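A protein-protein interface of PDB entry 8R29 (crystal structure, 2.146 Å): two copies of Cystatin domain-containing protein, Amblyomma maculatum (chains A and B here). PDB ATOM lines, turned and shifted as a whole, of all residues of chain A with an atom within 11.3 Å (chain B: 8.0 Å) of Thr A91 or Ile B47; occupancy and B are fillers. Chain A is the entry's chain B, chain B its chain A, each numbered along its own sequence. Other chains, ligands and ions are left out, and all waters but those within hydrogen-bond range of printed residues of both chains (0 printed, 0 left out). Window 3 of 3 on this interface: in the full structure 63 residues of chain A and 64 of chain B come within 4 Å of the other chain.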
ATOM      1  N   ARG A  60       1.610   8.382 -13.391  1.00  0.00           N
ATOM      2  CA  ARG A  60       1.741   6.965 -13.699  1.00  0.00           C
ATOM      3  C   ARG A  60       0.366   6.403 -13.984  1.00  0.00           C
ATOM      4  O   ARG A  60      -0.438   6.251 -13.064  1.00  0.00           O
ATOM      5  CB  ARG A  60       2.191   6.085 -12.541  1.00  0.00           C
ATOM      6  N   LEU A  61       0.110   6.142 -15.266  1.00  0.00           N
ATOM      7  CA  LEU A  61      -1.229   5.803 -15.715  1.00  0.00           C
ATOM      8  C   LEU A  61      -1.214   4.401 -16.301  1.00  0.00           C
ATOM      9  O   LEU A  61      -0.337   4.071 -17.093  1.00  0.00           O
ATOM     10  CB  LEU A  61      -1.651   6.828 -16.763  1.00  0.00           C
ATOM     11  CG  LEU A  61      -1.703   8.267 -16.275  1.00  0.00           C
ATOM     12  CD1 LEU A  61      -2.136   9.182 -17.406  1.00  0.00           C
ATOM     13  CD2 LEU A  61      -2.631   8.399 -15.075  1.00  0.00           C
ATOM     14  N   THR A  62      -2.223   3.606 -15.927  1.00  0.00           N
ATOM     15  CA  THR A  62      -2.422   2.284 -16.506  1.00  0.00           C
ATOM     16  C   THR A  62      -3.730   2.366 -17.270  1.00  0.00           C
ATOM     17  O   THR A  62      -4.648   3.043 -16.851  1.00  0.00           O
ATOM     18  CB  THR A  62      -2.301   1.193 -15.424  1.00  0.00           C
ATOM     19  OG1 THR A  62      -1.006   1.346 -14.830  1.00  0.00           O
ATOM     20  CG2 THR A  62      -2.433  -0.235 -15.921  1.00  0.00           C
ATOM     21  N   PHE A  63      -3.772   1.780 -18.454  1.00  0.00           N
ATOM     22  CA  PHE A  63      -4.946   1.934 -19.287  1.00  0.00           C
ATOM     23  C   PHE A  63      -5.015   0.820 -20.306  1.00  0.00           C
ATOM     24  O   PHE A  63      -3.995   0.267 -20.743  1.00  0.00           O
ATOM     25  CB  PHE A  63      -4.959   3.248 -20.068  1.00  0.00           C
ATOM     26  CG  PHE A  63      -3.642   3.674 -20.677  1.00  0.00           C
ATOM     27  CD1 PHE A  63      -2.720   4.404 -19.939  1.00  0.00           C
ATOM     28  CD2 PHE A  63      -3.327   3.350 -21.983  1.00  0.00           C
ATOM     29  CE1 PHE A  63      -1.510   4.791 -20.490  1.00  0.00           C
ATOM     30  CE2 PHE A  63      -2.111   3.741 -22.529  1.00  0.00           C
ATOM     31  CZ  PHE A  63      -1.194   4.452 -21.777  1.00  0.00           C
ATOM     32  N   LYS A  64      -6.254   0.537 -20.698  1.00  0.00           N
ATOM     33  CA  LYS A  64      -6.509  -0.447 -21.727  1.00  0.00           C
ATOM     34  C   LYS A  64      -6.497   0.253 -23.077  1.00  0.00           C
ATOM     35  O   LYS A  64      -7.082   1.317 -23.184  1.00  0.00           O
ATOM     36  CB  LYS A  64      -7.867  -1.100 -21.502  1.00  0.00           C
ATOM     37  CG  LYS A  64      -7.942  -2.095 -20.352  1.00  0.00           C
ATOM     38  CD  LYS A  64      -9.370  -2.557 -20.089  1.00  0.00           C
ATOM     39  CE  LYS A  64      -9.438  -3.909 -19.411  1.00  0.00           C
ATOM     40  NZ  LYS A  64     -10.831  -4.277 -19.073  1.00  0.00           N
ATOM     41  N   ILE A  65      -5.907  -0.407 -24.085  1.00  0.00           N
ATOM     42  CA  ILE A  65      -5.852   0.103 -25.443  1.00  0.00           C
ATOM     43  C   ILE A  65      -6.614  -0.785 -26.436  1.00  0.00           C
ATOM     44  O   ILE A  65      -6.899  -1.948 -26.202  1.00  0.00           O
ATOM     45  CB  ILE A  65      -4.384   0.275 -25.859  1.00  0.00           C
ATOM     46  CG1 ILE A  65      -3.656  -1.064 -26.019  1.00  0.00           C
ATOM     47  CG2 ILE A  65      -3.674   1.178 -24.859  1.00  0.00           C
ATOM     48  CD1 ILE A  65      -2.309  -0.929 -26.707  1.00  0.00           C
ATOM     49  N   ALA A  66      -6.963  -0.162 -27.561  1.00  0.00           N
ATOM     50  CA  ALA A  66      -7.521  -0.806 -28.730  1.00  0.00           C
ATOM     51  C   ALA A  66      -6.717  -0.359 -29.946  1.00  0.00           C
ATOM     52  O   ALA A  66      -6.020   0.640 -29.882  1.00  0.00           O
ATOM     53  CB  ALA A  66      -8.964  -0.427 -28.872  1.00  0.00           C
ATOM     54  N   GLU A  67      -6.773  -1.123 -31.031  1.00  0.00           N
ATOM     55  CA  GLU A  67      -6.176  -0.672 -32.265  1.00  0.00           C
ATOM     56  C   GLU A  67      -7.102   0.398 -32.805  1.00  0.00           C
ATOM     57  O   GLU A  67      -8.315   0.259 -32.698  1.00  0.00           O
ATOM     58  CB  GLU A  67      -6.035  -1.785 -33.296  1.00  0.00           C
ATOM     59  CG  GLU A  67      -5.336  -1.317 -34.558  1.00  0.00           C
ATOM     60  CD  GLU A  67      -5.456  -2.226 -35.769  1.00  0.00           C
ATOM     61  OE1 GLU A  67      -6.335  -3.109 -35.769  1.00  0.00           O
ATOM     62  OE2 GLU A  67      -4.688  -2.022 -36.730  1.00  0.00           O
ATOM     63  N   ASP A  87     -13.209  -3.469 -28.222  1.00  0.00           N
ATOM     64  CA  ASP A  87     -12.603  -4.710 -27.739  1.00  0.00           C
ATOM     65  C   ASP A  87     -11.137  -4.489 -27.370  1.00  0.00           C
ATOM     66  O   ASP A  87     -10.317  -4.139 -28.219  1.00  0.00           O
ATOM     67  CB  ASP A  87     -12.632  -5.822 -28.792  1.00  0.00           C
ATOM     68  N   VAL A  88     -10.812  -4.742 -26.102  1.00  0.00           N
ATOM     69  CA  VAL A  88      -9.473  -4.539 -25.574  1.00  0.00           C
ATOM     70  C   VAL A  88      -8.472  -5.379 -26.360  1.00  0.00           C
ATOM     71  O   VAL A  88      -8.770  -6.521 -26.695  1.00  0.00           O
ATOM     72  CB  VAL A  88      -9.433  -4.929 -24.087  1.00  0.00           C
ATOM     73  CG1 VAL A  88      -8.017  -4.908 -23.532  1.00  0.00           C
ATOM     74  CG2 VAL A  88     -10.368  -4.067 -23.253  1.00  0.00           C
ATOM     75  N   LYS A  89      -7.268  -4.834 -26.606  1.00  0.00           N
ATOM     76  CA  LYS A  89      -6.203  -5.616 -27.228  1.00  0.00           C
ATOM     77  C   LYS A  89      -4.968  -5.746 -26.330  1.00  0.00           C
ATOM     78  O   LYS A  89      -4.222  -6.704 -26.462  1.00  0.00           O
ATOM     79  CB  LYS A  89      -5.861  -5.096 -28.633  1.00  0.00           C
ATOM     80  CG  LYS A  89      -5.048  -3.816 -28.706  1.00  0.00           C
ATOM     81  CD  LYS A  89      -4.386  -3.620 -30.036  1.00  0.00           C
ATOM     82  CE  LYS A  89      -3.134  -4.455 -30.206  1.00  0.00           C
ATOM     83  NZ  LYS A  89      -2.380  -4.030 -31.409  1.00  0.00           N
ATOM     84  N   ASP A  90      -4.732  -4.817 -25.403  1.00  0.00           N
ATOM     85  CA  ASP A  90      -3.615  -4.921 -24.469  1.00  0.00           C
ATOM     86  C   ASP A  90      -3.892  -3.963 -23.311  1.00  0.00           C
ATOM     87  O   ASP A  90      -4.824  -3.174 -23.378  1.00  0.00           O
ATOM     88  CB  ASP A  90      -2.291  -4.646 -25.193  1.00  0.00           C
ATOM     89  CG  ASP A  90      -1.042  -5.221 -24.554  1.00  0.00           C
ATOM     90  OD1 ASP A  90      -1.156  -5.749 -23.423  1.00  0.00           O
ATOM     91  OD2 ASP A  90       0.046  -5.123 -25.204  1.00  0.00           O
ATOM     92  N   THR A  91      -3.133  -4.067 -22.228  1.00  0.00           N
ATOM     93  CA  THR A  91      -3.132  -3.044 -21.191  1.00  0.00           C
ATOM     94  C   THR A  91      -1.715  -2.476 -21.102  1.00  0.00           C
ATOM     95  O   THR A  91      -0.750  -3.231 -21.282  1.00  0.00           O
ATOM     96  CB  THR A  91      -3.690  -3.617 -19.881  1.00  0.00           C
ATOM     97  OG1 THR A  91      -5.029  -4.032 -20.162  1.00  0.00           O
ATOM     98  CG2 THR A  91      -3.710  -2.628 -18.738  1.00  0.00           C
ATOM     99  N   CYS A  92      -1.588  -1.153 -20.876  1.00  0.00           N
ATOM    100  CA  CYS A  92      -0.273  -0.520 -20.842  1.00  0.00           C
ATOM    101  C   CYS A  92      -0.130   0.429 -19.656  1.00  0.00           C
ATOM    102  O   CYS A  92      -1.108   0.953 -19.124  1.00  0.00           O
ATOM    103  CB  CYS A  92       0.002   0.256 -22.127  1.00  0.00           C
ATOM    104  SG  CYS A  92      -0.301  -0.709 -23.628  1.00  0.00           S
ATOM    105  N   THR A  93       1.118   0.664 -19.282  1.00  0.00           N
ATOM    106  CA  THR A  93       1.439   1.639 -18.258  1.00  0.00           C
ATOM    107  C   THR A  93       2.379   2.672 -18.837  1.00  0.00           C
ATOM    108  O   THR A  93       3.373   2.314 -19.459  1.00  0.00           O
ATOM    109  CB  THR A  93       2.075   0.984 -17.032  1.00  0.00           C
ATOM    110  OG1 THR A  93       0.957   0.412 -16.365  1.00  0.00           O
ATOM    111  CG2 THR A  93       2.823   1.941 -16.130  1.00  0.00           C
ATOM    112  N   ALA A  94       2.050   3.940 -18.591  1.00  0.00           N
ATOM    113  CA  ALA A  94       2.917   5.023 -18.994  1.00  0.00           C
ATOM    114  C   ALA A  94       3.182   5.928 -17.806  1.00  0.00           C
ATOM    115  O   ALA A  94       2.302   6.155 -16.976  1.00  0.00           O
ATOM    116  CB  ALA A  94       2.267   5.787 -20.124  1.00  0.00           C
ATOM    117  N   SER A 109       8.509   6.382 -19.607  1.00  0.00           N
ATOM    118  CA  SER A 109       8.388   4.959 -19.855  1.00  0.00           C
ATOM    119  C   SER A 109       7.023   4.656 -20.423  1.00  0.00           C
ATOM    120  O   SER A 109       6.064   5.267 -19.998  1.00  0.00           O
ATOM    121  CB  SER A 109       8.588   4.158 -18.587  1.00  0.00           C
ATOM    122  OG  SER A 109       7.626   4.514 -17.606  1.00  0.00           O
ATOM    123  N   PHE A 110       6.979   3.633 -21.283  1.00  0.00           N
ATOM    124  CA  PHE A 110       5.777   3.121 -21.919  1.00  0.00           C
ATOM    125  C   PHE A 110       5.982   1.623 -22.140  1.00  0.00           C
ATOM    126  O   PHE A 110       6.858   1.232 -22.915  1.00  0.00           O
ATOM    127  CB  PHE A 110       5.493   3.810 -23.255  1.00  0.00           C
ATOM    128  CG  PHE A 110       4.160   3.431 -23.860  1.00  0.00           C
ATOM    129  CD1 PHE A 110       4.001   2.253 -24.571  1.00  0.00           C
ATOM    130  CD2 PHE A 110       3.035   4.198 -23.605  1.00  0.00           C
ATOM    131  CE1 PHE A 110       2.755   1.880 -25.048  1.00  0.00           C
ATOM    132  CE2 PHE A 110       1.793   3.829 -24.090  1.00  0.00           C
ATOM    133  CZ  PHE A 110       1.652   2.665 -24.802  1.00  0.00           C
ATOM    134  N   THR A 111       5.188   0.798 -21.440  1.00  0.00           N
ATOM    135  CA  THR A 111       5.331  -0.645 -21.515  1.00  0.00           C
ATOM    136  C   THR A 111       3.946  -1.279 -21.490  1.00  0.00           C
ATOM    137  O   THR A 111       3.059  -0.767 -20.802  1.00  0.00           O
ATOM    138  CB  THR A 111       6.208  -1.160 -20.366  1.00  0.00           C
ATOM    139  OG1 THR A 111       6.227  -2.581 -20.494  1.00  0.00           O
ATOM    140  CG2 THR A 111       5.722  -0.745 -18.990  1.00  0.00           C
ATOM    141  N   CYS A 112       3.769  -2.398 -22.211  1.00  0.00           N
ATOM    142  CA  CYS A 112       2.460  -3.038 -22.256  1.00  0.00           C
ATOM    143  C   CYS A 112       2.465  -4.436 -21.629  1.00  0.00           C
ATOM    144  O   CYS A 112       2.173  -5.432 -22.290  1.00  0.00           O
ATOM    145  CB  CYS A 112       1.896  -3.018 -23.668  1.00  0.00           C
ATOM    146  SG  CYS A 112       1.596  -1.329 -24.249  1.00  0.00           S
ATOM    147  N   GLY A 113       2.707  -4.478 -20.312  1.00  0.00           N
ATOM    148  CA  GLY A 113       2.291  -5.592 -19.469  1.00  0.00           C
ATOM    149  C   GLY A 113       1.092  -5.220 -18.593  1.00  0.00           C
ATOM    150  O   GLY A 113       0.940  -4.074 -18.152  1.00  0.00           O
ATOM    151  N   VAL A 114       0.242  -6.213 -18.336  1.00  0.00           N
ATOM    152  CA  VAL A 114      -1.031  -5.985 -17.678  1.00  0.00           C
ATOM    153  C   VAL A 114      -1.027  -6.666 -16.313  1.00  0.00           C
ATOM    154  O   VAL A 114      -0.399  -7.705 -16.099  1.00  0.00           O
ATOM    155  CB  VAL A 114      -2.209  -6.483 -18.537  1.00  0.00           C
ATOM    156  N   ASN A 115      -1.772  -6.071 -15.380  1.00  0.00           N
ATOM    157  CA  ASN A 115      -1.654  -6.471 -13.998  1.00  0.00           C
ATOM    158  C   ASN A 115      -3.056  -6.517 -13.410  1.00  0.00           C
ATOM    159  O   ASN A 115      -3.879  -5.622 -13.645  1.00  0.00           O
ATOM    160  CB  ASN A 115      -0.667  -5.593 -13.219  1.00  0.00           C
ATOM    161  N   ALA A 116      -3.289  -7.648 -12.728  1.00  0.00           N
ATOM    162  CA  ALA A 116      -4.222  -7.752 -11.624  1.00  0.00           C
ATOM    163  C   ALA A 116      -3.461  -7.821 -10.293  1.00  0.00           C
ATOM    164  O   ALA A 116      -3.976  -8.402  -9.338  1.00  0.00           O
ATOM    165  CB  ALA A 116      -5.078  -8.975 -11.843  1.00  0.00           C
ATOM    166  N   ALA A 117      -2.244  -7.237 -10.243  1.00  0.00           N
ATOM    167  CA  ALA A 117      -1.421  -7.119  -9.041  1.00  0.00           C
ATOM    168  C   ALA A 117      -2.255  -7.255  -7.758  1.00  0.00           C
ATOM    169  O   ALA A 117      -1.649  -7.547  -6.703  1.00  0.00           O
ATOM    170  CB  ALA A 117      -0.710  -5.791  -9.051  1.00  0.00           C
ATOM    171  N   LYS B  14      -4.703   8.201  -7.241  1.00  0.00           N
ATOM    172  CA  LYS B  14      -5.790   9.140  -7.431  1.00  0.00           C
ATOM    173  C   LYS B  14      -6.986   8.370  -7.992  1.00  0.00           C
ATOM    174  O   LYS B  14      -6.821   7.246  -8.461  1.00  0.00           O
ATOM    175  CB  LYS B  14      -5.314  10.289  -8.328  1.00  0.00           C
ATOM    176  CG  LYS B  14      -4.201  11.145  -7.742  1.00  0.00           C
ATOM    177  CD  LYS B  14      -4.587  11.935  -6.507  1.00  0.00           C
ATOM    178  CE  LYS B  14      -3.423  12.778  -6.022  1.00  0.00           C
ATOM    179  NZ  LYS B  14      -3.768  13.571  -4.829  1.00  0.00           N
ATOM    180  N   PRO B  15      -8.233   8.900  -7.873  1.00  0.00           N
ATOM    181  CA  PRO B  15      -9.380   8.366  -8.614  1.00  0.00           C
ATOM    182  C   PRO B  15      -9.352   8.762 -10.089  1.00  0.00           C
ATOM    183  O   PRO B  15      -9.060   9.908 -10.406  1.00  0.00           O
ATOM    184  CB  PRO B  15     -10.592   9.030  -7.933  1.00  0.00           C
ATOM    185  CG  PRO B  15     -10.045  10.360  -7.413  1.00  0.00           C
ATOM    186  CD  PRO B  15      -8.618  10.037  -7.011  1.00  0.00           C
ATOM    187  N   VAL B  16      -9.703   7.811 -10.958  1.00  0.00           N
ATOM    188  CA  VAL B  16      -9.842   8.037 -12.383  1.00  0.00           C
ATOM    189  C   VAL B  16     -11.063   8.927 -12.636  1.00  0.00           C
ATOM    190  O   VAL B  16     -10.952   9.960 -13.294  1.00  0.00           O
ATOM    191  CB  VAL B  16      -9.931   6.705 -13.161  1.00  0.00           C
ATOM    192  CG1 VAL B  16      -9.891   6.938 -14.665  1.00  0.00           C
ATOM    193  CG2 VAL B  16      -8.852   5.703 -12.768  1.00  0.00           C
ATOM    194  N   ASP B  17     -12.239   8.498 -12.150  1.00  0.00           N
ATOM    195  CA  ASP B  17     -13.405   9.362 -12.007  1.00  0.00           C
ATOM    196  C   ASP B  17     -13.696  10.068 -13.315  1.00  0.00           C
ATOM    197  O   ASP B  17     -13.834   9.424 -14.348  1.00  0.00           O
ATOM    198  CB  ASP B  17     -13.182  10.453 -10.949  1.00  0.00           C
ATOM    199  N   PHE B  22      -6.184  12.973 -17.203  1.00  0.00           N
ATOM    200  CA  PHE B  22      -5.621  11.639 -17.241  1.00  0.00           C
ATOM    201  C   PHE B  22      -5.779  11.073 -18.645  1.00  0.00           C
ATOM    202  O   PHE B  22      -4.854  10.459 -19.198  1.00  0.00           O
ATOM    203  CB  PHE B  22      -6.246  10.714 -16.191  1.00  0.00           C
ATOM    204  CG  PHE B  22      -5.977  11.048 -14.739  1.00  0.00           C
ATOM    205  CD1 PHE B  22      -5.053  12.025 -14.358  1.00  0.00           C
ATOM    206  CD2 PHE B  22      -6.684  10.395 -13.731  1.00  0.00           C
ATOM    207  CE1 PHE B  22      -4.849  12.333 -13.019  1.00  0.00           C
ATOM    208  CE2 PHE B  22      -6.463  10.696 -12.394  1.00  0.00           C
ATOM    209  CZ  PHE B  22      -5.563  11.669 -12.036  1.00  0.00           C
ATOM    210  N   VAL B  43      -6.784   4.910 -26.730  1.00  0.00           N
ATOM    211  CA  VAL B  43      -7.190   4.602 -25.367  1.00  0.00           C
ATOM    212  C   VAL B  43      -8.637   4.166 -25.385  1.00  0.00           C
ATOM    213  O   VAL B  43      -9.460   4.925 -25.850  1.00  0.00           O
ATOM    214  CB  VAL B  43      -7.055   5.830 -24.453  1.00  0.00           C
ATOM    215  CG1 VAL B  43      -7.649   5.575 -23.075  1.00  0.00           C
ATOM    216  CG2 VAL B  43      -5.598   6.311 -24.382  1.00  0.00           C
ATOM    217  N   LEU B  44      -8.926   2.993 -24.824  1.00  0.00           N
ATOM    218  CA  LEU B  44     -10.281   2.587 -24.471  1.00  0.00           C
ATOM    219  C   LEU B  44     -10.641   3.116 -23.080  1.00  0.00           C
ATOM    220  O   LEU B  44     -11.669   3.758 -22.905  1.00  0.00           O
ATOM    221  CB  LEU B  44     -10.365   1.059 -24.520  1.00  0.00           C
ATOM    222  N   GLU B  45      -9.798   2.845 -22.072  1.00  0.00           N
ATOM    223  CA  GLU B  45     -10.001   3.486 -20.782  1.00  0.00           C
ATOM    224  C   GLU B  45      -8.758   3.399 -19.907  1.00  0.00           C
ATOM    225  O   GLU B  45      -7.982   2.431 -19.991  1.00  0.00           O
ATOM    226  CB  GLU B  45     -11.169   2.850 -20.023  1.00  0.00           C
ATOM    227  CG  GLU B  45     -10.994   1.362 -19.786  1.00  0.00           C
ATOM    228  CD  GLU B  45     -12.108   0.731 -18.971  1.00  0.00           C
ATOM    229  OE1 GLU B  45     -12.911   1.492 -18.349  1.00  0.00           O
ATOM    230  OE2 GLU B  45     -12.178  -0.522 -18.979  1.00  0.00           O
ATOM    231  N   VAL B  46      -8.680   4.391 -19.007  1.00  0.00           N
ATOM    232  CA  VAL B  46      -7.717   4.410 -17.924  1.00  0.00           C
ATOM    233  C   VAL B  46      -8.331   3.707 -16.724  1.00  0.00           C
ATOM    234  O   VAL B  46      -9.505   3.888 -16.447  1.00  0.00           O
ATOM    235  CB  VAL B  46      -7.325   5.858 -17.573  1.00  0.00           C
ATOM    236  CG1 VAL B  46      -6.241   5.880 -16.512  1.00  0.00           C
ATOM    237  CG2 VAL B  46      -6.909   6.664 -18.807  1.00  0.00           C
ATOM    238  N   ILE B  47      -7.509   2.960 -15.978  1.00  0.00           N
ATOM    239  CA  ILE B  47      -8.013   2.093 -14.916  1.00  0.00           C
ATOM    240  C   ILE B  47      -7.264   2.328 -13.601  1.00  0.00           C
ATOM    241  O   ILE B  47      -7.852   2.071 -12.551  1.00  0.00           O
ATOM    242  CB  ILE B  47      -7.953   0.615 -15.352  1.00  0.00           C
ATOM    243  CG1 ILE B  47      -6.524   0.179 -15.700  1.00  0.00           C
ATOM    244  CG2 ILE B  47      -8.915   0.377 -16.507  1.00  0.00           C
ATOM    245  CD1 ILE B  47      -6.418  -1.186 -16.314  1.00  0.00           C
ATOM    246  N   ASP B  48      -5.973   2.722 -13.654  1.00  0.00           N
ATOM    247  CA  ASP B  48      -5.239   3.185 -12.483  1.00  0.00           C
ATOM    248  C   ASP B  48      -4.504   4.477 -12.840  1.00  0.00           C
ATOM    249  O   ASP B  48      -4.153   4.714 -14.007  1.00  0.00           O
ATOM    250  CB  ASP B  48      -4.271   2.126 -11.942  1.00  0.00           C
ATOM    251  N   ALA B  49      -4.286   5.305 -11.807  1.00  0.00           N
ATOM    252  CA  ALA B  49      -3.647   6.607 -11.948  1.00  0.00           C
ATOM    253  C   ALA B  49      -2.946   6.986 -10.643  1.00  0.00           C
ATOM    254  O   ALA B  49      -3.574   6.973  -9.588  1.00  0.00           O
ATOM    255  CB  ALA B  49      -4.678   7.642 -12.333  1.00  0.00           C
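The backbone carbonyl oxygen (O) of Asp B48 sits at hydrogen-bond distance from the backbone NH (N) of Thr A62. The backbone NH of Leu B44 lies within hydrogen-bond range of the backbone carbonyl oxygen of Lys A64, 3.0 Å away. OE2 of Glu B45 lies within salt-bridge range of NZ of Lys A64 (3.99 Å). The backbone NH (N) of Ile B47 sits at hydrogen-bond distance from the backbone carbonyl oxygen (O) of Thr A62 (3.0 Å).
Arg A60 touches Ala B49 (O to CA, 3.4 Å). Leu A61 touches Phe B22 (CD1 to O, 3.5 Å). Asp B48 touches Leu A61 (O to CA, 3.6 Å). Leu A61 touches Ala B49. O of Thr A62 touches CG1 of Val B46, 3.3 Å away. Phe A63 touches Glu B45 (CB to O, 3.1 Å). Val B46 touches Phe A63. Lys A64 touches Val B43 (O to C, 3.9 Å). CD1 of Ile B47 touches CG2 of Thr A91, 3.9 Å away.
The side-chain sulfur of Cys A112 forms a disulfide with the side-chain sulfur of Cys A92 (2.1 Å). The backbone carbonyl oxygen (O) of Ala B49 sits at hydrogen-bond distance from the backbone NH (N) of Lys B14, at 2.9 Å. The backbone NH (N) of Cys A92 is in hydrogen-bond range of the backbone carbonyl oxygen (O) of Phe A63. The backbone NH (N) of Leu A61 lies within hydrogen-bond range of the backbone carbonyl oxygen (O) of Ala A94 (2.8 Å). OG1 of Thr A62 sits at hydrogen-bond distance from OG1 of Thr A93 (2.7 Å).
No position is printed for both chains. Of the 13 pairs that touch across the chains among the printed residues, none has its exchanged pair printed and touching as well.
Printed residues of chain B that touch a printed residue of chain A: Phe B22, Val B43, Leu B44, Glu B45, Val B46, Ile B47, Asp B48 and Ala B49. Printed residues of chain A that touch a printed residue of chain B: Arg A60, Leu A61, Thr A62, Phe A63, Lys A64 and Thr A91. Hydrophobic or aromatic side chains of chain A that line the printed part of chain B: Leu A61 and Phe A63. Among the printed residues, 13 pairs touch across the chains.
Printed residues of chain B within 4 Å of Leu A61: Phe B22 (3.5 Å), Asp B48 (3.6 Å) and Ala B49 (3.5 Å). Of chain B, only Ile B47 comes within 4 Å of Thr A91. Asn A115 touches none of the printed residues of chain B. Of the printed residues of chain A, Val B43 touches Lys A64 (3.9 Å). Of the printed residues of chain A, Leu B44 touches Lys A64. Of the printed residues of chain A, Glu B45 touches Phe A63 and Lys A64. Val B46 touches two residues of chain A. Of chain A, only Thr A62 and Thr A91 come within 4 Å of Ile B47. The nearest residue of chain B that does not touch Thr A91 is Glu B45 (6.7 Å). The nearest residue of chain A that does not touch Ile B47 is Phe A63 (4.2 Å). The nearest printed residue of chain B that does not touch Thr A62 is Glu B45 (4.6 Å).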
